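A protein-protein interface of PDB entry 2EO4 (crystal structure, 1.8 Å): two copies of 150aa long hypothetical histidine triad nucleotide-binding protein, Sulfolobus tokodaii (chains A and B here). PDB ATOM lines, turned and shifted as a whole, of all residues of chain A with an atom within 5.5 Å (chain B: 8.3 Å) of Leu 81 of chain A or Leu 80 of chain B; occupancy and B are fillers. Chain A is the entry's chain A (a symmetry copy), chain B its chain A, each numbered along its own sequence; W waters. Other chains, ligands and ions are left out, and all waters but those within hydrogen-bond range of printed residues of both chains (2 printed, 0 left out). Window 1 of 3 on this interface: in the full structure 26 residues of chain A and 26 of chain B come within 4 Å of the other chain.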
ATOM      1  N   TYR A  47      -6.774  -1.246   3.381  1.00  0.00           N
ATOM      2  CA  TYR A  47      -6.429  -1.457   4.785  1.00  0.00           C
ATOM      3  C   TYR A  47      -7.637  -1.664   5.703  1.00  0.00           C
ATOM      4  O   TYR A  47      -7.603  -2.492   6.613  1.00  0.00           O
ATOM      5  CB  TYR A  47      -5.602  -0.256   5.270  1.00  0.00           C
ATOM      6  CG  TYR A  47      -4.932  -0.430   6.616  1.00  0.00           C
ATOM      7  CD1 TYR A  47      -5.620  -0.183   7.804  1.00  0.00           C
ATOM      8  CD2 TYR A  47      -3.596  -0.821   6.698  1.00  0.00           C
ATOM      9  CE1 TYR A  47      -4.992  -0.316   9.042  1.00  0.00           C
ATOM     10  CE2 TYR A  47      -2.959  -0.958   7.929  1.00  0.00           C
ATOM     11  CZ  TYR A  47      -3.659  -0.703   9.094  1.00  0.00           C
ATOM     12  OH  TYR A  47      -3.026  -0.835  10.308  1.00  0.00           O
ATOM     13  N   ARG A  79       9.951   5.840   3.851  1.00  0.00           N
ATOM     14  CA  ARG A  79       8.590   6.360   3.914  1.00  0.00           C
ATOM     15  C   ARG A  79       7.692   5.132   3.787  1.00  0.00           C
ATOM     16  O   ARG A  79       7.811   4.389   2.817  1.00  0.00           O
ATOM     17  CB  ARG A  79       8.298   7.291   2.728  1.00  0.00           C
ATOM     18  CG  ARG A  79       9.136   8.559   2.643  1.00  0.00           C
ATOM     19  CD  ARG A  79       9.033   9.179   1.246  1.00  0.00           C
ATOM     20  NE  ARG A  79       7.648   9.427   0.846  1.00  0.00           N
ATOM     21  CZ  ARG A  79       7.257   9.655  -0.405  1.00  0.00           C
ATOM     22  NH1 ARG A  79       8.145   9.669  -1.392  1.00  0.00           N
ATOM     23  NH2 ARG A  79       5.972   9.862  -0.673  1.00  0.00           N
ATOM     24  N   LEU A  80       6.818   4.909   4.766  1.00  0.00           N
ATOM     25  CA  LEU A  80       5.886   3.783   4.717  1.00  0.00           C
ATOM     26  C   LEU A  80       4.487   4.352   4.532  1.00  0.00           C
ATOM     27  O   LEU A  80       4.099   5.285   5.238  1.00  0.00           O
ATOM     28  CB  LEU A  80       5.905   2.983   6.017  1.00  0.00           C
ATOM     29  CG  LEU A  80       7.244   2.429   6.492  1.00  0.00           C
ATOM     30  CD1 LEU A  80       7.004   1.473   7.650  1.00  0.00           C
ATOM     31  CD2 LEU A  80       7.952   1.740   5.351  1.00  0.00           C
ATOM     32  N   LEU A  81       3.728   3.808   3.591  1.00  0.00           N
ATOM     33  CA  LEU A  81       2.380   4.320   3.398  1.00  0.00           C
ATOM     34  C   LEU A  81       1.443   3.357   2.701  1.00  0.00           C
ATOM     35  O   LEU A  81       1.863   2.436   2.003  1.00  0.00           O
ATOM     36  CB  LEU A  81       2.408   5.627   2.604  1.00  0.00           C
ATOM     37  CG  LEU A  81       2.865   5.551   1.144  1.00  0.00           C
ATOM     38  CD1 LEU A  81       2.250   6.699   0.358  1.00  0.00           C
ATOM     39  CD2 LEU A  81       4.382   5.602   1.071  1.00  0.00           C
ATOM     40  N   THR A  82       0.152   3.568   2.927  1.00  0.00           N
ATOM     41  CA  THR A  82      -0.855   2.765   2.269  1.00  0.00           C
ATOM     42  C   THR A  82      -2.004   3.714   2.003  1.00  0.00           C
ATOM     43  O   THR A  82      -2.326   4.570   2.835  1.00  0.00           O
ATOM     44  CB  THR A  82      -1.313   1.558   3.127  1.00  0.00           C
ATOM     45  OG1 THR A  82      -2.191   0.739   2.343  1.00  0.00           O
ATOM     46  CG2 THR A  82      -2.009   2.014   4.403  1.00  0.00           C
ATOM     47  N   ASN A  83      -2.603   3.572   0.829  1.00  0.00           N
ATOM     48  CA  ASN A  83      -3.692   4.445   0.422  1.00  0.00           C
ATOM     49  C   ASN A  83      -5.028   3.738   0.386  1.00  0.00           C
ATOM     50  O   ASN A  83      -5.122   2.589  -0.040  1.00  0.00           O
ATOM     51  CB  ASN A  83      -3.382   5.029  -0.954  1.00  0.00           C
ATOM     52  CG  ASN A  83      -2.087   5.802  -0.967  1.00  0.00           C
ATOM     53  OD1 ASN A  83      -1.885   6.694  -0.145  1.00  0.00           O
ATOM     54  ND2 ASN A  83      -1.200   5.471  -1.908  1.00  0.00           N
ATOM     55  N   ILE A  84      -6.063   4.441   0.833  1.00  0.00           N
ATOM     56  CA  ILE A  84      -7.415   3.897   0.862  1.00  0.00           C
ATOM     57  C   ILE A  84      -8.314   4.795   0.022  1.00  0.00           C
ATOM     58  O   ILE A  84      -8.627   5.911   0.424  1.00  0.00           O
ATOM     59  CB  ILE A  84      -7.962   3.861   2.303  1.00  0.00           C
ATOM     60  CG1 ILE A  84      -7.059   2.992   3.184  1.00  0.00           C
ATOM     61  CG2 ILE A  84      -9.383   3.315   2.307  1.00  0.00           C
ATOM     62  CD1 ILE A  84      -7.241   3.249   4.679  1.00  0.00           C
ATOM     63  N   HIS A  96      -1.785  -2.991   0.014  1.00  0.00           N
ATOM     64  CA  HIS A  96      -0.337  -3.049  -0.052  1.00  0.00           C
ATOM     65  C   HIS A  96       0.259  -1.844   0.637  1.00  0.00           C
ATOM     66  O   HIS A  96      -0.312  -0.750   0.613  1.00  0.00           O
ATOM     67  CB  HIS A  96       0.166  -3.122  -1.497  1.00  0.00           C
ATOM     68  CG  HIS A  96      -0.265  -1.978  -2.361  1.00  0.00           C
ATOM     69  ND1 HIS A  96      -1.574  -1.786  -2.747  1.00  0.00           N
ATOM     70  CD2 HIS A  96       0.453  -1.006  -2.972  1.00  0.00           C
ATOM     71  CE1 HIS A  96      -1.643  -0.748  -3.562  1.00  0.00           C
ATOM     72  NE2 HIS A  96      -0.426  -0.258  -3.716  1.00  0.00           N
ATOM     73  N   VAL A  97       1.406  -2.067   1.265  1.00  0.00           N
ATOM     74  CA  VAL A  97       2.122  -1.012   1.967  1.00  0.00           C
ATOM     75  C   VAL A  97       3.370  -0.680   1.171  1.00  0.00           C
ATOM     76  O   VAL A  97       4.135  -1.573   0.806  1.00  0.00           O
ATOM     77  CB  VAL A  97       2.548  -1.474   3.379  1.00  0.00           C
ATOM     78  CG1 VAL A  97       3.414  -0.407   4.042  1.00  0.00           C
ATOM     79  CG2 VAL A  97       1.310  -1.746   4.225  1.00  0.00           C
ATOM     80  N   HIS A  98       3.562   0.604   0.890  1.00  0.00           N
ATOM     81  CA  HIS A  98       4.733   1.058   0.153  1.00  0.00           C
ATOM     82  C   HIS A  98       5.895   1.283   1.114  1.00  0.00           C
ATOM     83  O   HIS A  98       5.704   1.828   2.195  1.00  0.00           O
ATOM     84  CB  HIS A  98       4.461   2.409  -0.522  1.00  0.00           C
ATOM     85  CG  HIS A  98       3.415   2.370  -1.589  1.00  0.00           C
ATOM     86  ND1 HIS A  98       3.724   2.240  -2.926  1.00  0.00           N
ATOM     87  CD2 HIS A  98       2.068   2.497  -1.525  1.00  0.00           C
ATOM     88  CE1 HIS A  98       2.612   2.290  -3.640  1.00  0.00           C
ATOM     89  NE2 HIS A  98       1.593   2.445  -2.814  1.00  0.00           N
ATOM     90  N   ILE A  99       7.091   0.857   0.709  1.00  0.00           N
ATOM     91  CA  ILE A  99       8.302   1.108   1.480  1.00  0.00           C
ATOM     92  C   ILE A  99       9.157   1.840   0.452  1.00  0.00           C
ATOM     93  O   ILE A  99       9.646   1.238  -0.508  1.00  0.00           O
ATOM     94  CB  ILE A  99       9.037  -0.179   1.916  1.00  0.00           C
ATOM     95  CG1 ILE A  99       8.142  -1.019   2.827  1.00  0.00           C
ATOM     96  CG2 ILE A  99      10.311   0.199   2.696  1.00  0.00           C
ATOM     97  CD1 ILE A  99       8.770  -2.368   3.226  1.00  0.00           C
ATOM     98  N   ILE A 100       9.313   3.145   0.651  1.00  0.00           N
ATOM     99  CA  ILE A 100      10.064   3.995  -0.267  1.00  0.00           C
ATOM    100  C   ILE A 100      11.319   4.543   0.412  1.00  0.00           C
ATOM    101  O   ILE A 100      11.240   5.401   1.290  1.00  0.00           O
ATOM    102  CB  ILE A 100       9.176   5.173  -0.736  1.00  0.00           C
ATOM    103  CG1 ILE A 100       7.905   4.621  -1.391  1.00  0.00           C
ATOM    104  CG2 ILE A 100       9.944   6.058  -1.718  1.00  0.00           C
ATOM    105  CD1 ILE A 100       6.875   5.690  -1.754  1.00  0.00           C
ATOM    106  N   THR B  36      -5.257  13.166  11.796  1.00  0.00           N
ATOM    107  CA  THR B  36      -4.998  12.631  13.127  1.00  0.00           C
ATOM    108  C   THR B  36      -3.730  11.792  13.180  1.00  0.00           C
ATOM    109  O   THR B  36      -3.304  11.227  12.172  1.00  0.00           O
ATOM    110  CB  THR B  36      -6.197  11.766  13.579  1.00  0.00           C
ATOM    111  OG1 THR B  36      -7.347  12.604  13.710  1.00  0.00           O
ATOM    112  CG2 THR B  36      -5.915  11.067  14.911  1.00  0.00           C
ATOM    113  N   VAL B  38      -1.859   8.607  15.229  1.00  0.00           N
ATOM    114  CA  VAL B  38      -2.081   7.479  16.124  1.00  0.00           C
ATOM    115  C   VAL B  38      -0.716   7.122  16.680  1.00  0.00           C
ATOM    116  O   VAL B  38       0.240   6.930  15.927  1.00  0.00           O
ATOM    117  CB  VAL B  38      -2.665   6.263  15.383  1.00  0.00           C
ATOM    118  CG1 VAL B  38      -2.912   5.127  16.372  1.00  0.00           C
ATOM    119  CG2 VAL B  38      -3.964   6.654  14.692  1.00  0.00           C
ATOM    120  N   ALA B  59      -1.437  -1.345  14.559  1.00  0.00           N
ATOM    121  CA  ALA B  59      -2.155  -1.541  13.302  1.00  0.00           C
ATOM    122  C   ALA B  59      -3.660  -1.650  13.535  1.00  0.00           C
ATOM    123  O   ALA B  59      -4.458  -1.145  12.747  1.00  0.00           O
ATOM    124  CB  ALA B  59      -1.648  -2.792  12.598  1.00  0.00           C
ATOM    125  N   VAL B  62      -5.034   1.784  14.462  1.00  0.00           N
ATOM    126  CA  VAL B  62      -5.088   2.597  13.252  1.00  0.00           C
ATOM    127  C   VAL B  62      -6.352   2.260  12.451  1.00  0.00           C
ATOM    128  O   VAL B  62      -7.027   3.152  11.939  1.00  0.00           O
ATOM    129  CB  VAL B  62      -3.827   2.373  12.383  1.00  0.00           C
ATOM    130  CG1 VAL B  62      -4.009   3.002  11.000  1.00  0.00           C
ATOM    131  CG2 VAL B  62      -2.627   3.005  13.068  1.00  0.00           C
ATOM    132  N   LYS B  63      -6.691   0.979  12.357  1.00  0.00           N
ATOM    133  CA  LYS B  63      -7.904   0.610  11.618  1.00  0.00           C
ATOM    134  C   LYS B  63      -9.147   1.229  12.262  1.00  0.00           C
ATOM    135  O   LYS B  63      -9.957   1.865  11.588  1.00  0.00           O
ATOM    136  CB  LYS B  63      -8.088  -0.910  11.562  1.00  0.00           C
ATOM    137  CG  LYS B  63      -9.380  -1.318  10.835  1.00  0.00           C
ATOM    138  CD  LYS B  63      -9.600  -2.829  10.795  1.00  0.00           C
ATOM    139  CE  LYS B  63     -10.949  -3.154  10.155  1.00  0.00           C
ATOM    140  NZ  LYS B  63     -11.196  -4.622  10.004  1.00  0.00           N
ATOM    141  N   VAL B  65      -9.503   3.790  14.436  1.00  0.00           N
ATOM    142  CA  VAL B  65      -9.521   5.240  14.350  1.00  0.00           C
ATOM    143  C   VAL B  65      -9.779   5.712  12.922  1.00  0.00           C
ATOM    144  O   VAL B  65     -10.506   6.682  12.715  1.00  0.00           O
ATOM    145  CB  VAL B  65      -8.204   5.838  14.885  1.00  0.00           C
ATOM    146  CG1 VAL B  65      -8.206   7.358  14.723  1.00  0.00           C
ATOM    147  CG2 VAL B  65      -8.045   5.467  16.358  1.00  0.00           C
ATOM    148  N   SER B  66      -9.196   5.026  11.941  1.00  0.00           N
ATOM    149  CA  SER B  66      -9.400   5.393  10.543  1.00  0.00           C
ATOM    150  C   SER B  66     -10.881   5.243  10.184  1.00  0.00           C
ATOM    151  O   SER B  66     -11.463   6.121   9.547  1.00  0.00           O
ATOM    152  CB  SER B  66      -8.548   4.516   9.617  1.00  0.00           C
ATOM    153  OG  SER B  66      -7.161   4.800   9.769  1.00  0.00           O
ATOM    154  N   LEU B  67     -11.489   4.127  10.579  1.00  0.00           N
ATOM    155  CA  LEU B  67     -12.906   3.926  10.288  1.00  0.00           C
ATOM    156  C   LEU B  67     -13.712   5.047  10.938  1.00  0.00           C
ATOM    157  O   LEU B  67     -14.634   5.597  10.331  1.00  0.00           O
ATOM    158  CB  LEU B  67     -13.376   2.566  10.813  1.00  0.00           C
ATOM    159  CG  LEU B  67     -12.949   1.350   9.983  1.00  0.00           C
ATOM    160  CD1 LEU B  67     -13.246   0.062  10.737  1.00  0.00           C
ATOM    161  CD2 LEU B  67     -13.678   1.374   8.643  1.00  0.00           C
ATOM    162  N   ILE B  69     -12.735   8.160  11.783  1.00  0.00           N
ATOM    163  CA  ILE B  69     -12.536   9.434  11.105  1.00  0.00           C
ATOM    164  C   ILE B  69     -13.261   9.481   9.763  1.00  0.00           C
ATOM    165  O   ILE B  69     -13.919  10.474   9.446  1.00  0.00           O
ATOM    166  CB  ILE B  69     -11.034   9.713  10.873  1.00  0.00           C
ATOM    167  CG1 ILE B  69     -10.332   9.911  12.219  1.00  0.00           C
ATOM    168  CG2 ILE B  69     -10.857  10.954   9.990  1.00  0.00           C
ATOM    169  CD1 ILE B  69      -8.808   9.986  12.127  1.00  0.00           C
ATOM    170  N   GLY B  77     -11.718   8.888   1.054  1.00  0.00           N
ATOM    171  CA  GLY B  77     -10.487   8.128   1.152  1.00  0.00           C
ATOM    172  C   GLY B  77      -9.640   8.570   2.327  1.00  0.00           C
ATOM    173  O   GLY B  77      -9.969   9.536   3.019  1.00  0.00           O
ATOM    174  N   LEU B  78      -8.547   7.850   2.553  1.00  0.00           N
ATOM    175  CA  LEU B  78      -7.628   8.162   3.643  1.00  0.00           C
ATOM    176  C   LEU B  78      -6.220   7.776   3.228  1.00  0.00           C
ATOM    177  O   LEU B  78      -6.026   6.767   2.556  1.00  0.00           O
ATOM    178  CB  LEU B  78      -7.968   7.359   4.899  1.00  0.00           C
ATOM    179  CG  LEU B  78      -9.353   7.481   5.538  1.00  0.00           C
ATOM    180  CD1 LEU B  78      -9.483   6.402   6.611  1.00  0.00           C
ATOM    181  CD2 LEU B  78      -9.547   8.869   6.129  1.00  0.00           C
ATOM    182  N   ARG B  79      -5.253   8.592   3.635  1.00  0.00           N
ATOM    183  CA  ARG B  79      -3.843   8.327   3.373  1.00  0.00           C
ATOM    184  C   ARG B  79      -3.248   7.972   4.734  1.00  0.00           C
ATOM    185  O   ARG B  79      -3.359   8.760   5.670  1.00  0.00           O
ATOM    186  CB  ARG B  79      -3.131   9.584   2.853  1.00  0.00           C
ATOM    187  CG  ARG B  79      -3.620  10.134   1.520  1.00  0.00           C
ATOM    188  CD  ARG B  79      -3.123  11.567   1.316  1.00  0.00           C
ATOM    189  NE  ARG B  79      -1.669  11.676   1.437  1.00  0.00           N
ATOM    190  CZ  ARG B  79      -1.014  12.821   1.617  1.00  0.00           C
ATOM    191  NH1 ARG B  79      -1.679  13.967   1.700  1.00  0.00           N
ATOM    192  NH2 ARG B  79       0.310  12.819   1.725  1.00  0.00           N
ATOM    193  N   LEU B  80      -2.644   6.792   4.850  1.00  0.00           N
ATOM    194  CA  LEU B  80      -2.008   6.378   6.100  1.00  0.00           C
ATOM    195  C   LEU B  80      -0.505   6.349   5.863  1.00  0.00           C
ATOM    196  O   LEU B  80      -0.046   5.790   4.866  1.00  0.00           O
ATOM    197  CB  LEU B  80      -2.450   4.976   6.517  1.00  0.00           C
ATOM    198  CG  LEU B  80      -3.945   4.720   6.674  1.00  0.00           C
ATOM    199  CD1 LEU B  80      -4.150   3.359   7.322  1.00  0.00           C
ATOM    200  CD2 LEU B  80      -4.575   5.818   7.496  1.00  0.00           C
ATOM    201  N   LEU B  81       0.264   6.947   6.762  1.00  0.00           N
ATOM    202  CA  LEU B  81       1.706   6.926   6.573  1.00  0.00           C
ATOM    203  C   LEU B  81       2.503   7.160   7.838  1.00  0.00           C
ATOM    204  O   LEU B  81       2.014   7.721   8.817  1.00  0.00           O
ATOM    205  CB  LEU B  81       2.129   7.967   5.535  1.00  0.00           C
ATOM    206  CG  LEU B  81       1.941   9.441   5.905  1.00  0.00           C
ATOM    207  CD1 LEU B  81       2.939  10.291   5.132  1.00  0.00           C
ATOM    208  CD2 LEU B  81       0.517   9.876   5.599  1.00  0.00           C
ATOM    209  N   THR B  82       3.744   6.690   7.814  1.00  0.00           N
ATOM    210  CA  THR B  82       4.639   6.906   8.931  1.00  0.00           C
ATOM    211  C   THR B  82       6.006   7.094   8.310  1.00  0.00           C
ATOM    212  O   THR B  82       6.362   6.415   7.340  1.00  0.00           O
ATOM    213  CB  THR B  82       4.638   5.725   9.934  1.00  0.00           C
ATOM    214  OG1 THR B  82       5.428   6.086  11.075  1.00  0.00           O
ATOM    215  CG2 THR B  82       5.176   4.450   9.297  1.00  0.00           C
ATOM    216  N   ASN B  83       6.759   8.037   8.859  1.00  0.00           N
ATOM    217  CA  ASN B  83       8.077   8.357   8.335  1.00  0.00           C
ATOM    218  C   ASN B  83       9.195   7.926   9.259  1.00  0.00           C
ATOM    219  O   ASN B  83       9.094   8.061  10.476  1.00  0.00           O
ATOM    220  CB  ASN B  83       8.167   9.859   8.084  1.00  0.00           C
ATOM    221  CG  ASN B  83       7.114  10.341   7.119  1.00  0.00           C
ATOM    222  OD1 ASN B  83       6.979   9.801   6.021  1.00  0.00           O
ATOM    223  ND2 ASN B  83       6.361  11.369   7.516  1.00  0.00           N
ATOM    224  N   HIS B  96       4.593   7.584  15.145  1.00  0.00           N
ATOM    225  CA  HIS B  96       3.209   7.973  14.954  1.00  0.00           C
ATOM    226  C   HIS B  96       2.796   7.718  13.523  1.00  0.00           C
ATOM    227  O   HIS B  96       3.601   7.844  12.596  1.00  0.00           O
ATOM    228  CB  HIS B  96       2.975   9.445  15.307  1.00  0.00           C
ATOM    229  CG  HIS B  96       3.811  10.410  14.526  1.00  0.00           C
ATOM    230  ND1 HIS B  96       5.176  10.511  14.683  1.00  0.00           N
ATOM    231  CD2 HIS B  96       3.463  11.366  13.633  1.00  0.00           C
ATOM    232  CE1 HIS B  96       5.632  11.493  13.924  1.00  0.00           C
ATOM    233  NE2 HIS B  96       4.613  12.028  13.278  1.00  0.00           N
ATOM    234  N   VAL B  97       1.534   7.343  13.362  1.00  0.00           N
ATOM    235  CA  VAL B  97       0.968   7.072  12.048  1.00  0.00           C
ATOM    236  C   VAL B  97      -0.001   8.190  11.713  1.00  0.00           C
ATOM    237  O   VAL B  97      -0.874   8.522  12.516  1.00  0.00           O
ATOM    238  CB  VAL B  97       0.196   5.733  12.041  1.00  0.00           C
ATOM    239  CG1 VAL B  97      -0.503   5.536  10.698  1.00  0.00           C
ATOM    240  CG2 VAL B  97       1.161   4.583  12.304  1.00  0.00           C
ATOM    241  N   HIS B  98       0.166   8.777  10.534  1.00  0.00           N
ATOM    242  CA  HIS B  98      -0.712   9.848  10.083  1.00  0.00           C
ATOM    243  C   HIS B  98      -1.944   9.256   9.408  1.00  0.00           C
ATOM    244  O   HIS B  98      -1.832   8.304   8.644  1.00  0.00           O
ATOM    245  CB  HIS B  98      -0.014  10.716   9.027  1.00  0.00           C
ATOM    246  CG  HIS B  98       1.171  11.475   9.532  1.00  0.00           C
ATOM    247  ND1 HIS B  98       1.089  12.786   9.947  1.00  0.00           N
ATOM    248  CD2 HIS B  98       2.475  11.127   9.641  1.00  0.00           C
ATOM    249  CE1 HIS B  98       2.292  13.214  10.289  1.00  0.00           C
ATOM    250  NE2 HIS B  98       3.151  12.227  10.113  1.00  0.00           N
ATOM    251  N   ILE B  99      -3.112   9.828   9.699  1.00  0.00           N
ATOM    252  CA  ILE B  99      -4.352   9.434   9.040  1.00  0.00           C
ATOM    253  C   ILE B  99      -4.810  10.766   8.457  1.00  0.00           C
ATOM    254  O   ILE B  99      -5.242  11.660   9.190  1.00  0.00           O
ATOM    255  CB  ILE B  99      -5.433   8.915  10.012  1.00  0.00           C
ATOM    256  CG1 ILE B  99      -4.940   7.661  10.735  1.00  0.00           C
ATOM    257  CG2 ILE B  99      -6.703   8.554   9.219  1.00  0.00           C
ATOM    258  CD1 ILE B  99      -5.927   7.138  11.796  1.00  0.00           C
ATOM    259  N   ILE B 100      -4.690  10.895   7.141  1.00  0.00           N
ATOM    260  CA  ILE B 100      -5.042  12.124   6.436  1.00  0.00           C
ATOM    261  C   ILE B 100      -6.236  11.892   5.511  1.00  0.00           C
ATOM    262  O   ILE B 100      -6.121  11.226   4.484  1.00  0.00           O
ATOM    263  CB  ILE B 100      -3.833  12.616   5.604  1.00  0.00           C
ATOM    264  CG1 ILE B 100      -2.629  12.821   6.529  1.00  0.00           C
ATOM    265  CG2 ILE B 100      -4.181  13.917   4.881  1.00  0.00           C
ATOM    266  CD1 ILE B 100      -1.330  13.155   5.798  1.00  0.00           C
ATOM    267  N   PRO B 101      -7.406  12.440   5.872  1.00  0.00           N
ATOM    268  CA  PRO B 101      -8.621  12.278   5.064  1.00  0.00           C
ATOM    269  C   PRO B 101      -8.582  12.963   3.704  1.00  0.00           C
ATOM    270  O   PRO B 101      -7.961  14.014   3.536  1.00  0.00           O
ATOM    271  CB  PRO B 101      -9.714  12.875   5.956  1.00  0.00           C
ATOM    272  CG  PRO B 101      -9.173  12.685   7.350  1.00  0.00           C
ATOM    273  CD  PRO B 101      -7.722  13.075   7.163  1.00  0.00           C
ATOM    274  N   THR B 102      -9.256  12.357   2.735  1.00  0.00           N
ATOM    275  CA  THR B 102      -9.334  12.918   1.395  1.00  0.00           C
ATOM    276  C   THR B 102     -10.778  12.834   0.910  1.00  0.00           C
ATOM    277  O   THR B 102     -11.572  12.048   1.430  1.00  0.00           O
ATOM    278  CB  THR B 102      -8.421  12.162   0.395  1.00  0.00           C
ATOM    279  OG1 THR B 102      -8.849  10.801   0.271  1.00  0.00           O
ATOM    280  CG2 THR B 102      -6.974  12.192   0.868  1.00  0.00           C
HETATM  281  O   HOH W   1       5.634   7.967   4.218  1.00  0.00           O
HETATM  282  O   HOH W   2      -0.700   7.694   2.308  1.00  0.00           O
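O of Val 62 of chain B lies within hydrogen-bond range of OG of Ser 66 of chain B (2.7 Å). The backbone carbonyl oxygen of Gly 77 of chain B is in hydrogen-bond range of the backbone NH of Thr 102 of chain B, 2.9 Å away. The backbone carbonyl oxygen (O) of Leu 81 of chain B lies within hydrogen-bond range of the backbone NH (N) of His 98 of chain B, 2.7 Å away. OG1 of Thr 82 of chain B is in hydrogen-bond range of O of His 96 of chain B, 3.0 Å away. N of His 98 of chain A is in hydrogen-bond range of O of Leu 81 of chain A, at 2.7 Å. OG1 of Thr 82 of chain A sits at hydrogen-bond distance from O of His 96 of chain A (3.0 Å).
O of Ala 59 of chain B sits at hydrogen-bond distance from OH of Tyr 47 of chain A (2.8 Å). O of Ile 84 of chain A lies within hydrogen-bond range of N of Leu 78 of chain B (2.9 Å). The backbone NH of Thr 82 of chain A sits at hydrogen-bond distance from the backbone carbonyl oxygen of Leu 80 of chain B (3.0 Å). N of Thr 82 of chain B sits at hydrogen-bond distance from O of Leu 80 of chain A, at 3.0 Å.
Of chain A, only Tyr 47 (3.9 Å), Leu 81 (3.2 Å) and Thr 82 (3.0 Å) come within 4 Å of Leu 80 of chain B. Printed residues of chain A within 4 Å of Leu 81 of chain B: Leu 80 and Leu 81. Printed residues of chain A within 4 Å of Ala 59 of chain B: Tyr 47 (2.8 Å). Of the printed residues of chain A, Val 62 of chain B touches Tyr 47 (3.9 Å). Of the printed residues of chain B, Leu 80 of chain A touches Leu 81 (3.2 Å) and Thr 82 (3.0 Å). Val 65 of chain B touches none of the printed residues of chain A. The nearest residue of chain B that does not touch Leu 81 of chain A is Thr 82 of chain B (5.1 Å). The nearest printed residue of chain B that does not touch Thr 82 of chain A is Arg 79 of chain B (4.004 Å).
Water W2 lies within hydrogen-bond range of the side-chain amide oxygen of Asn 83 of chain A (2.9 Å) and the backbone carbonyl oxygen of Leu 80 of chain B (3.3 Å). Water W1 lies within hydrogen-bond range of the side-chain amide oxygen of Asn 83 of chain B (2.9 Å) and the backbone carbonyl oxygen of Leu 80 of chain A (3.3 Å).
Leu 80 of chain A touches Leu 81 of chain B, and with the chains exchanged Leu 81 of chain A touches Leu 80 of chain B. Leu 80 of chain A touches Thr 82 of chain B, and with the chains exchanged Thr 82 of chain A touches Leu 80 of chain B. Leu 81 of chain A touches its own counterpart, Leu 81 of chain B. Positions printed for both chains: 79, 80, 81, 82, 83, 96, 97, 98, 99 and 100. Of the 12 pairs that touch across the chains among the printed residues, 5 have their exchanged pair printed and touching as well.
Tyr 47 of chain A touches Val 62 of chain B. Lys 63 of chain B touches Tyr 47 of chain A. Tyr 47 of chain A touches Leu 80 of chain B. Leu 80 of chain A touches Leu 81 of chain B. Leu 81 of chain A touches Leu 80 of chain B (CA to O, 3.2 Å). CB of Leu 81 of chain A touches CB of Leu 81 of chain B (3.8 Å). Leu 78 of chain B touches Asn 83 of chain A. Gly 77 of chain B touches Ile 84 of chain A (CA to O, 3.0 Å).
Along chain A the printed residues that touch a printed residue of chain B span positions 47 to 84. Printed residues of chain B that touch a printed residue of chain A: Ala 59, Val 62, Lys 63, Gly 77, Leu 78, Leu 80, Leu 81 and Thr 82. Hydrophobic or aromatic side chains of chain B within 4 Å of the printed part of chain A: Ala 59, Val 62, Leu 80 and Leu 81.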
